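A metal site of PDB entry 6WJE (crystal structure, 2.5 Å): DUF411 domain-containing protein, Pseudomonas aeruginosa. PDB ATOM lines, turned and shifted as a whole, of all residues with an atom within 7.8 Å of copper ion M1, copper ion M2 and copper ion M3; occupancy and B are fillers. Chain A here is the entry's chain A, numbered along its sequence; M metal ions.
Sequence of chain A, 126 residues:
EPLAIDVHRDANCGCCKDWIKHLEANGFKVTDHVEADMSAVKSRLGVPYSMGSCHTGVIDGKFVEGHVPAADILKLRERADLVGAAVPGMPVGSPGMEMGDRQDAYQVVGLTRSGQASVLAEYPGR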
ATOM      1  N   VAL A   7     -31.683  22.126  -5.679  1.00  0.00           N
ATOM      2  CA  VAL A   7     -30.592  21.252  -6.099  1.00  0.00           C
ATOM      3  C   VAL A   7     -29.667  22.022  -7.039  1.00  0.00           C
ATOM      4  O   VAL A   7     -30.154  22.720  -7.935  1.00  0.00           O
ATOM      5  CB  VAL A   7     -31.121  19.963  -6.760  1.00  0.00           C
ATOM      6  CG1 VAL A   7     -29.979  19.059  -7.219  1.00  0.00           C
ATOM      7  CG2 VAL A   7     -31.967  19.224  -5.744  1.00  0.00           C
ATOM      8  N   HIS A   8     -28.358  21.953  -6.788  1.00  0.00           N
ATOM      9  CA  HIS A   8     -27.348  22.448  -7.712  1.00  0.00           C
ATOM     10  C   HIS A   8     -26.603  21.238  -8.258  1.00  0.00           C
ATOM     11  O   HIS A   8     -26.265  20.310  -7.505  1.00  0.00           O
ATOM     12  CB  HIS A   8     -26.310  23.433  -7.061  1.00  0.00           C
ATOM     13  CG  HIS A   8     -26.898  24.747  -6.554  1.00  0.00           C
ATOM     14  ND1 HIS A   8     -26.502  26.009  -7.001  1.00  0.00           N
ATOM     15  CD2 HIS A   8     -27.827  24.969  -5.608  1.00  0.00           C
ATOM     16  CE1 HIS A   8     -27.199  26.929  -6.361  1.00  0.00           C
ATOM     17  NE2 HIS A   8     -27.997  26.320  -5.506  1.00  0.00           N
ATOM     18  N   ARG A   9     -26.336  21.225  -9.559  1.00  0.00           N
ATOM     19  CA  ARG A   9     -25.627  20.118 -10.179  1.00  0.00           C
ATOM     20  C   ARG A   9     -25.050  20.584 -11.499  1.00  0.00           C
ATOM     21  O   ARG A   9     -25.436  21.616 -12.047  1.00  0.00           O
ATOM     22  CB  ARG A   9     -26.532  18.905 -10.385  1.00  0.00           C
ATOM     23  CG  ARG A   9     -27.838  19.234 -11.029  1.00  0.00           C
ATOM     24  CD  ARG A   9     -27.781  18.898 -12.439  1.00  0.00           C
ATOM     25  NE  ARG A   9     -29.027  19.196 -13.121  1.00  0.00           N
ATOM     26  CZ  ARG A   9     -29.147  19.197 -14.457  1.00  0.00           C
ATOM     27  NH1 ARG A   9     -28.084  18.920 -15.216  1.00  0.00           N
ATOM     28  NH2 ARG A   9     -30.315  19.469 -15.017  1.00  0.00           N
ATOM     29  N   ASP A  10     -24.116  19.781 -12.010  1.00  0.00           N
ATOM     30  CA  ASP A  10     -23.494  20.029 -13.302  1.00  0.00           C
ATOM     31  C   ASP A  10     -24.431  19.706 -14.471  1.00  0.00           C
ATOM     32  O   ASP A  10     -25.325  18.851 -14.380  1.00  0.00           O
ATOM     33  CB  ASP A  10     -22.208  19.195 -13.382  1.00  0.00           C
ATOM     34  CG  ASP A  10     -21.430  19.408 -14.663  1.00  0.00           C
ATOM     35  OD1 ASP A  10     -20.667  20.408 -14.749  1.00  0.00           O
ATOM     36  OD2 ASP A  10     -21.571  18.553 -15.572  1.00  0.00           O
ATOM     37  N   CYS A  13     -24.635  15.912 -15.643  1.00  0.00           N
ATOM     38  CA  CYS A  13     -24.797  14.888 -14.589  1.00  0.00           C
ATOM     39  C   CYS A  13     -26.175  14.297 -14.780  1.00  0.00           C
ATOM     40  O   CYS A  13     -27.167  14.801 -14.251  1.00  0.00           O
ATOM     41  CB  CYS A  13     -24.599  15.422 -13.169  1.00  0.00           C
ATOM     42  SG  CYS A  13     -24.689  14.073 -11.824  1.00  0.00           S
ATOM     43  N   GLY A  14     -26.215  13.205 -15.521  1.00  0.00           N
ATOM     44  CA  GLY A  14     -27.449  12.544 -15.808  1.00  0.00           C
ATOM     45  C   GLY A  14     -28.026  11.768 -14.639  1.00  0.00           C
ATOM     46  O   GLY A  14     -29.240  11.778 -14.468  1.00  0.00           O
ATOM     47  N   CYS A  15     -27.205  11.019 -13.897  1.00  0.00           N
ATOM     48  CA  CYS A  15     -27.718  10.458 -12.659  1.00  0.00           C
ATOM     49  C   CYS A  15     -28.383  11.522 -11.802  1.00  0.00           C
ATOM     50  O   CYS A  15     -29.496  11.305 -11.305  1.00  0.00           O
ATOM     51  CB  CYS A  15     -26.626   9.673 -11.904  1.00  0.00           C
ATOM     52  SG  CYS A  15     -25.156  10.641 -11.439  1.00  0.00           S
ATOM     53  N   CYS A  16     -27.742  12.680 -11.658  1.00  0.00           N
ATOM     54  CA  CYS A  16     -28.335  13.772 -10.875  1.00  0.00           C
ATOM     55  C   CYS A  16     -29.724  14.150 -11.385  1.00  0.00           C
ATOM     56  O   CYS A  16     -30.631  14.413 -10.581  1.00  0.00           O
ATOM     57  CB  CYS A  16     -27.440  15.022 -10.877  1.00  0.00           C
ATOM     58  SG  CYS A  16     -25.768  14.752 -10.209  1.00  0.00           S
ATOM     59  N   LYS A  17     -29.927  14.160 -12.714  1.00  0.00           N
ATOM     60  CA  LYS A  17     -31.253  14.452 -13.230  1.00  0.00           C
ATOM     61  C   LYS A  17     -32.241  13.346 -12.882  1.00  0.00           C
ATOM     62  O   LYS A  17     -33.410  13.617 -12.577  1.00  0.00           O
ATOM     63  CB  LYS A  17     -31.227  14.641 -14.737  1.00  0.00           C
ATOM     64  CG  LYS A  17     -30.495  15.841 -15.296  1.00  0.00           C
ATOM     65  CD  LYS A  17     -30.456  15.718 -16.847  1.00  0.00           C
ATOM     66  CE  LYS A  17     -29.533  16.721 -17.543  1.00  0.00           C
ATOM     67  N   ASP A  18     -31.753  12.103 -12.907  1.00  0.00           N
ATOM     68  CA  ASP A  18     -32.612  10.916 -12.579  1.00  0.00           C
ATOM     69  C   ASP A  18     -33.111  11.049 -11.132  1.00  0.00           C
ATOM     70  O   ASP A  18     -34.310  10.818 -10.907  1.00  0.00           O
ATOM     71  CB  ASP A  18     -31.837   9.613 -12.800  1.00  0.00           C
ATOM     72  CG  ASP A  18     -32.713   8.374 -12.709  1.00  0.00           C
ATOM     73  OD1 ASP A  18     -33.938   8.496 -12.945  1.00  0.00           O
ATOM     74  OD2 ASP A  18     -32.176   7.297 -12.390  1.00  0.00           O
ATOM     75  N   TRP A  19     -32.210  11.402 -10.215  1.00  0.00           N
ATOM     76  CA  TRP A  19     -32.540  11.568  -8.798  1.00  0.00           C
ATOM     77  C   TRP A  19     -33.611  12.631  -8.598  1.00  0.00           C
ATOM     78  O   TRP A  19     -34.557  12.420  -7.834  1.00  0.00           O
ATOM     79  CB  TRP A  19     -31.274  11.925  -8.010  1.00  0.00           C
ATOM     80  CG  TRP A  19     -31.440  12.133  -6.511  1.00  0.00           C
ATOM     81  CD1 TRP A  19     -31.617  11.147  -5.563  1.00  0.00           C
ATOM     82  CD2 TRP A  19     -31.415  13.367  -5.786  1.00  0.00           C
ATOM     83  NE1 TRP A  19     -31.690  11.699  -4.308  1.00  0.00           N
ATOM     84  CE2 TRP A  19     -31.582  13.066  -4.423  1.00  0.00           C
ATOM     85  CE3 TRP A  19     -31.252  14.698  -6.172  1.00  0.00           C
ATOM     86  CZ2 TRP A  19     -31.590  14.048  -3.428  1.00  0.00           C
ATOM     87  CZ3 TRP A  19     -31.267  15.685  -5.192  1.00  0.00           C
ATOM     88  CH2 TRP A  19     -31.442  15.350  -3.831  1.00  0.00           C
ATOM     89  N   LYS A  42     -20.612  23.170  -2.129  1.00  0.00           N
ATOM     90  CA  LYS A  42     -20.347  22.270  -1.007  1.00  0.00           C
ATOM     91  C   LYS A  42     -19.602  22.999   0.101  1.00  0.00           C
ATOM     92  O   LYS A  42     -19.819  22.730   1.304  1.00  0.00           O
ATOM     93  CB  LYS A  42     -19.550  21.062  -1.483  1.00  0.00           C
ATOM     94  CG  LYS A  42     -20.323  20.092  -2.339  1.00  0.00           C
ATOM     95  CD  LYS A  42     -19.379  19.154  -3.049  1.00  0.00           C
ATOM     96  CE  LYS A  42     -19.969  18.626  -4.360  1.00  0.00           C
ATOM     97  NZ  LYS A  42     -21.309  17.971  -4.172  1.00  0.00           N
ATOM     98  N   SER A  53     -20.142  14.154  -3.190  1.00  0.00           N
ATOM     99  CA  SER A  53     -20.872  13.391  -4.183  1.00  0.00           C
ATOM    100  C   SER A  53     -21.106  14.262  -5.416  1.00  0.00           C
ATOM    101  O   SER A  53     -20.475  15.305  -5.588  1.00  0.00           O
ATOM    102  CB  SER A  53     -22.196  12.882  -3.604  1.00  0.00           C
ATOM    103  OG  SER A  53     -22.614  11.750  -4.324  1.00  0.00           O
ATOM    104  N   CYS A  54     -21.968  13.784  -6.314  1.00  0.00           N
ATOM    105  CA  CYS A  54     -22.235  14.396  -7.612  1.00  0.00           C
ATOM    106  C   CYS A  54     -23.126  15.635  -7.541  1.00  0.00           C
ATOM    107  O   CYS A  54     -23.172  16.376  -8.518  1.00  0.00           O
ATOM    108  CB  CYS A  54     -22.833  13.383  -8.581  1.00  0.00           C
ATOM    109  SG  CYS A  54     -24.134  12.397  -7.911  1.00  0.00           S
ATOM    110  N   HIS A  55     -23.939  15.806  -6.493  1.00  0.00           N
ATOM    111  CA  HIS A  55     -24.856  16.937  -6.497  1.00  0.00           C
ATOM    112  C   HIS A  55     -25.051  17.334  -5.044  1.00  0.00           C
ATOM    113  O   HIS A  55     -24.877  16.518  -4.137  1.00  0.00           O
ATOM    114  CB  HIS A  55     -26.195  16.616  -7.167  1.00  0.00           C
ATOM    115  CG  HIS A  55     -27.013  15.602  -6.429  1.00  0.00           C
ATOM    116  ND1 HIS A  55     -27.194  14.301  -6.869  1.00  0.00           N
ATOM    117  CD2 HIS A  55     -27.760  15.709  -5.307  1.00  0.00           C
ATOM    118  CE1 HIS A  55     -27.953  13.640  -6.018  1.00  0.00           C
ATOM    119  NE2 HIS A  55     -28.323  14.477  -5.067  1.00  0.00           N
ATOM    120  N   THR A  56     -25.514  18.583  -4.835  1.00  0.00           N
ATOM    121  CA  THR A  56     -25.772  19.114  -3.498  1.00  0.00           C
ATOM    122  C   THR A  56     -27.120  19.804  -3.449  1.00  0.00           C
ATOM    123  O   THR A  56     -27.345  20.794  -4.157  1.00  0.00           O
ATOM    124  CB  THR A  56     -24.693  20.121  -3.071  1.00  0.00           C
ATOM    125  OG1 THR A  56     -23.400  19.522  -3.223  1.00  0.00           O
ATOM    126  CG2 THR A  56     -24.878  20.516  -1.616  1.00  0.00           C
ATOM    127  N   GLU A  65     -26.526  15.694   0.410  1.00  0.00           N
ATOM    128  CA  GLU A  65     -25.391  15.418  -0.466  1.00  0.00           C
ATOM    129  C   GLU A  65     -25.549  14.039  -1.104  1.00  0.00           C
ATOM    130  O   GLU A  65     -25.475  13.018  -0.413  1.00  0.00           O
ATOM    131  CB  GLU A  65     -24.077  15.483   0.289  1.00  0.00           C
ATOM    132  CG  GLU A  65     -22.902  15.290  -0.649  1.00  0.00           C
ATOM    133  CD  GLU A  65     -22.552  16.560  -1.452  1.00  0.00           C
ATOM    134  OE1 GLU A  65     -23.043  17.653  -1.114  1.00  0.00           O
ATOM    135  OE2 GLU A  65     -21.795  16.453  -2.446  1.00  0.00           O
ATOM    136  N   GLY A  66     -25.675  14.019  -2.439  1.00  0.00           N
ATOM    137  CA  GLY A  66     -25.745  12.795  -3.193  1.00  0.00           C
ATOM    138  C   GLY A  66     -27.136  12.172  -3.224  1.00  0.00           C
ATOM    139  O   GLY A  66     -28.150  12.805  -2.938  1.00  0.00           O
ATOM    140  N   HIS A  67     -27.148  10.889  -3.580  1.00  0.00           N
ATOM    141  CA  HIS A  67     -28.372  10.152  -3.926  1.00  0.00           C
ATOM    142  C   HIS A  67     -29.038   9.623  -2.662  1.00  0.00           C
ATOM    143  O   HIS A  67     -29.134   8.412  -2.442  1.00  0.00           O
ATOM    144  CB  HIS A  67     -28.045   9.011  -4.880  1.00  0.00           C
ATOM    145  CG  HIS A  67     -27.640   9.477  -6.236  1.00  0.00           C
ATOM    146  ND1 HIS A  67     -28.532   9.582  -7.278  1.00  0.00           N
ATOM    147  CD2 HIS A  67     -26.470   9.997  -6.683  1.00  0.00           C
ATOM    148  CE1 HIS A  67     -27.909  10.065  -8.339  1.00  0.00           C
ATOM    149  NE2 HIS A  67     -26.655  10.336  -8.002  1.00  0.00           N
ATOM    150  N   GLY A  89     -20.008   9.633  -2.712  1.00  0.00           N
ATOM    151  CA  GLY A  89     -19.743   8.902  -3.951  1.00  0.00           C
ATOM    152  C   GLY A  89     -21.007   8.669  -4.756  1.00  0.00           C
ATOM    153  O   GLY A  89     -21.969   9.454  -4.691  1.00  0.00           O
ATOM    154  N   MET A  90     -21.055   7.552  -5.482  1.00  0.00           N
ATOM    155  CA  MET A  90     -22.184   7.223  -6.368  1.00  0.00           C
ATOM    156  C   MET A  90     -22.476   5.726  -6.350  1.00  0.00           C
ATOM    157  O   MET A  90     -22.281   5.034  -7.344  1.00  0.00           O
ATOM    158  CB  MET A  90     -21.917   7.720  -7.791  1.00  0.00           C
ATOM    159  CG  MET A  90     -22.112   9.223  -7.956  1.00  0.00           C
ATOM    160  SD  MET A  90     -22.008   9.861  -9.642  1.00  0.00           S
ATOM    161  CE  MET A  90     -20.918   8.632 -10.349  1.00  0.00           C
ATOM    162  N   PRO A  91     -23.002   5.202  -5.240  1.00  0.00           N
ATOM    163  CA  PRO A  91     -23.269   3.758  -5.161  1.00  0.00           C
ATOM    164  C   PRO A  91     -24.359   3.325  -6.135  1.00  0.00           C
ATOM    165  O   PRO A  91     -25.382   3.989  -6.266  1.00  0.00           O
ATOM    166  CB  PRO A  91     -23.707   3.562  -3.700  1.00  0.00           C
ATOM    167  CG  PRO A  91     -24.157   4.897  -3.239  1.00  0.00           C
ATOM    168  CD  PRO A  91     -23.327   5.912  -3.989  1.00  0.00           C
ATOM    169  N   VAL A  92     -24.088   2.254  -6.887  1.00  0.00           N
ATOM    170  CA  VAL A  92     -25.092   1.732  -7.818  1.00  0.00           C
ATOM    171  C   VAL A  92     -26.286   1.197  -7.047  1.00  0.00           C
ATOM    172  O   VAL A  92     -26.141   0.430  -6.076  1.00  0.00           O
ATOM    173  CB  VAL A  92     -24.460   0.673  -8.726  1.00  0.00           C
ATOM    174  CG1 VAL A  92     -25.395   0.214  -9.858  1.00  0.00           C
ATOM    175  CG2 VAL A  92     -23.218   1.252  -9.337  1.00  0.00           C
ATOM    176  N   SER A  94     -28.566   3.201  -5.638  1.00  0.00           N
ATOM    177  CA  SER A  94     -29.201   4.285  -4.933  1.00  0.00           C
ATOM    178  C   SER A  94     -30.107   4.988  -5.940  1.00  0.00           C
ATOM    179  O   SER A  94     -29.918   4.848  -7.152  1.00  0.00           O
ATOM    180  CB  SER A  94     -28.185   5.241  -4.323  1.00  0.00           C
ATOM    181  OG  SER A  94     -27.422   5.916  -5.312  1.00  0.00           O
ATOM    182  N   PRO A  95     -31.113   5.727  -5.473  1.00  0.00           N
ATOM    183  CA  PRO A  95     -32.093   6.306  -6.405  1.00  0.00           C
ATOM    184  C   PRO A  95     -31.444   7.289  -7.372  1.00  0.00           C
ATOM    185  O   PRO A  95     -30.729   8.204  -6.962  1.00  0.00           O
ATOM    186  CB  PRO A  95     -33.089   7.007  -5.471  1.00  0.00           C
ATOM    187  CG  PRO A  95     -32.861   6.437  -4.128  1.00  0.00           C
ATOM    188  CD  PRO A  95     -31.447   6.001  -4.062  1.00  0.00           C
ATOM    189  N   GLY A  96     -31.720   7.116  -8.661  1.00  0.00           N
ATOM    190  CA  GLY A  96     -31.062   7.884  -9.696  1.00  0.00           C
ATOM    191  C   GLY A  96     -29.757   7.299 -10.160  1.00  0.00           C
ATOM    192  O   GLY A  96     -29.184   7.791 -11.157  1.00  0.00           O
ATOM    193  N   MET A  97     -29.256   6.268  -9.484  1.00  0.00           N
ATOM    194  CA  MET A  97     -28.054   5.561  -9.887  1.00  0.00           C
ATOM    195  C   MET A  97     -28.344   4.086 -10.175  1.00  0.00           C
ATOM    196  O   MET A  97     -27.433   3.247 -10.196  1.00  0.00           O
ATOM    197  CB  MET A  97     -26.973   5.702  -8.794  1.00  0.00           C
ATOM    198  CG  MET A  97     -26.015   6.914  -8.984  1.00  0.00           C
ATOM    199  SD  MET A  97     -25.064   6.856 -10.532  1.00  0.00           S
ATOM    200  CE  MET A  97     -23.986   5.447 -10.334  1.00  0.00           C
ATOM    201  N   GLU A  98     -29.607   3.749 -10.425  1.00  0.00           N
ATOM    202  CA  GLU A  98     -30.018   2.357 -10.543  1.00  0.00           C
ATOM    203  C   GLU A  98     -29.582   1.779 -11.896  1.00  0.00           C
ATOM    204  O   GLU A  98     -29.773   2.391 -12.948  1.00  0.00           O
ATOM    205  CB  GLU A  98     -31.547   2.268 -10.314  1.00  0.00           C
ATOM    206  CG  GLU A  98     -32.527   2.567 -11.486  1.00  0.00           C
ATOM    207  CD  GLU A  98     -33.065   4.029 -11.653  1.00  0.00           C
ATOM    208  OE1 GLU A  98     -32.712   4.993 -10.925  1.00  0.00           O
ATOM    209  OE2 GLU A  98     -33.927   4.218 -12.558  1.00  0.00           O
ATOM    210  N   MET A  99     -28.945   0.625 -11.869  1.00  0.00           N
ATOM    211  CA  MET A  99     -28.369   0.070 -13.083  1.00  0.00           C
ATOM    212  C   MET A  99     -28.582  -1.437 -13.117  1.00  0.00           C
ATOM    213  O   MET A  99     -27.666  -2.226 -13.356  1.00  0.00           O
ATOM    214  CB  MET A  99     -26.905   0.444 -13.181  1.00  0.00           C
ATOM    215  CG  MET A  99     -26.673   1.630 -14.029  1.00  0.00           C
ATOM    216  SD  MET A  99     -25.036   2.207 -13.652  1.00  0.00           S
ATOM    217  CE  MET A  99     -25.475   3.824 -13.082  1.00  0.00           C
HETATM  218 CU    CU M   1     -25.277  11.167  -9.268  1.00  0.00          CU
HETATM  219 CU    CU M   2     -25.733  13.731  -8.290  1.00  0.00          CU
HETATM  220 CU    CU M   3     -23.781   8.774 -10.880  1.00  0.00          CU
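Copper ion M2 is bound by ND1 of His 55 (2.1 Å), SG of Cys 54 (2.1 Å) and SG of Cys 16 (2.2 Å).
Copper ion M2 has three donor atoms within binding distance.
Of the 29 residues printed, 3 come within 4 Å of copper ion M3.
Residues that only touch copper ion M2: Cys 13 (3.7 Å).
Of the 29 residues printed, 5 come within 4 Å of copper ion M2.
The nearest printed residue that does not touch copper ion M2 is Cys 15 (4.4 Å).
Copper ion M1 is bound by a ring nitrogen (NE2) of His 67 (2.0 Å), the side-chain sulfur (SG) of Cys 54 (2.2 Å) and the side-chain sulfur (SG) of Cys 15 (2.2 Å).
Copper ion M1 has three donor atoms within binding distance.
ND1 of His 67 sits at hydrogen-bond distance from O of Pro 95 (2.6 Å).
O of Gly 66 lies within hydrogen-bond range of NE2 of His 55 (2.7 Å).
The side-chain sulfur of Cys 13 is disulfide-bonded to the side-chain sulfur of Cys 16 (2.1 Å).
The side-chain sulfur (SG) of Cys 13 sits close to the side-chain sulfur (SG) of Cys 15.
Copper ion M3 is bound by SD of Met 97, SG of Cys 15 and SD of Met 90.
SG of Cys 13 touches copper ion M1, 3.9 Å away.
Within 4 Å of copper ion M1: Cys 13, Cys 15, Cys 16, Cys 54, His 67 and Met 90.
Along chain A the residues within 4 Å of copper ion M1 span positions 13 to 90.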
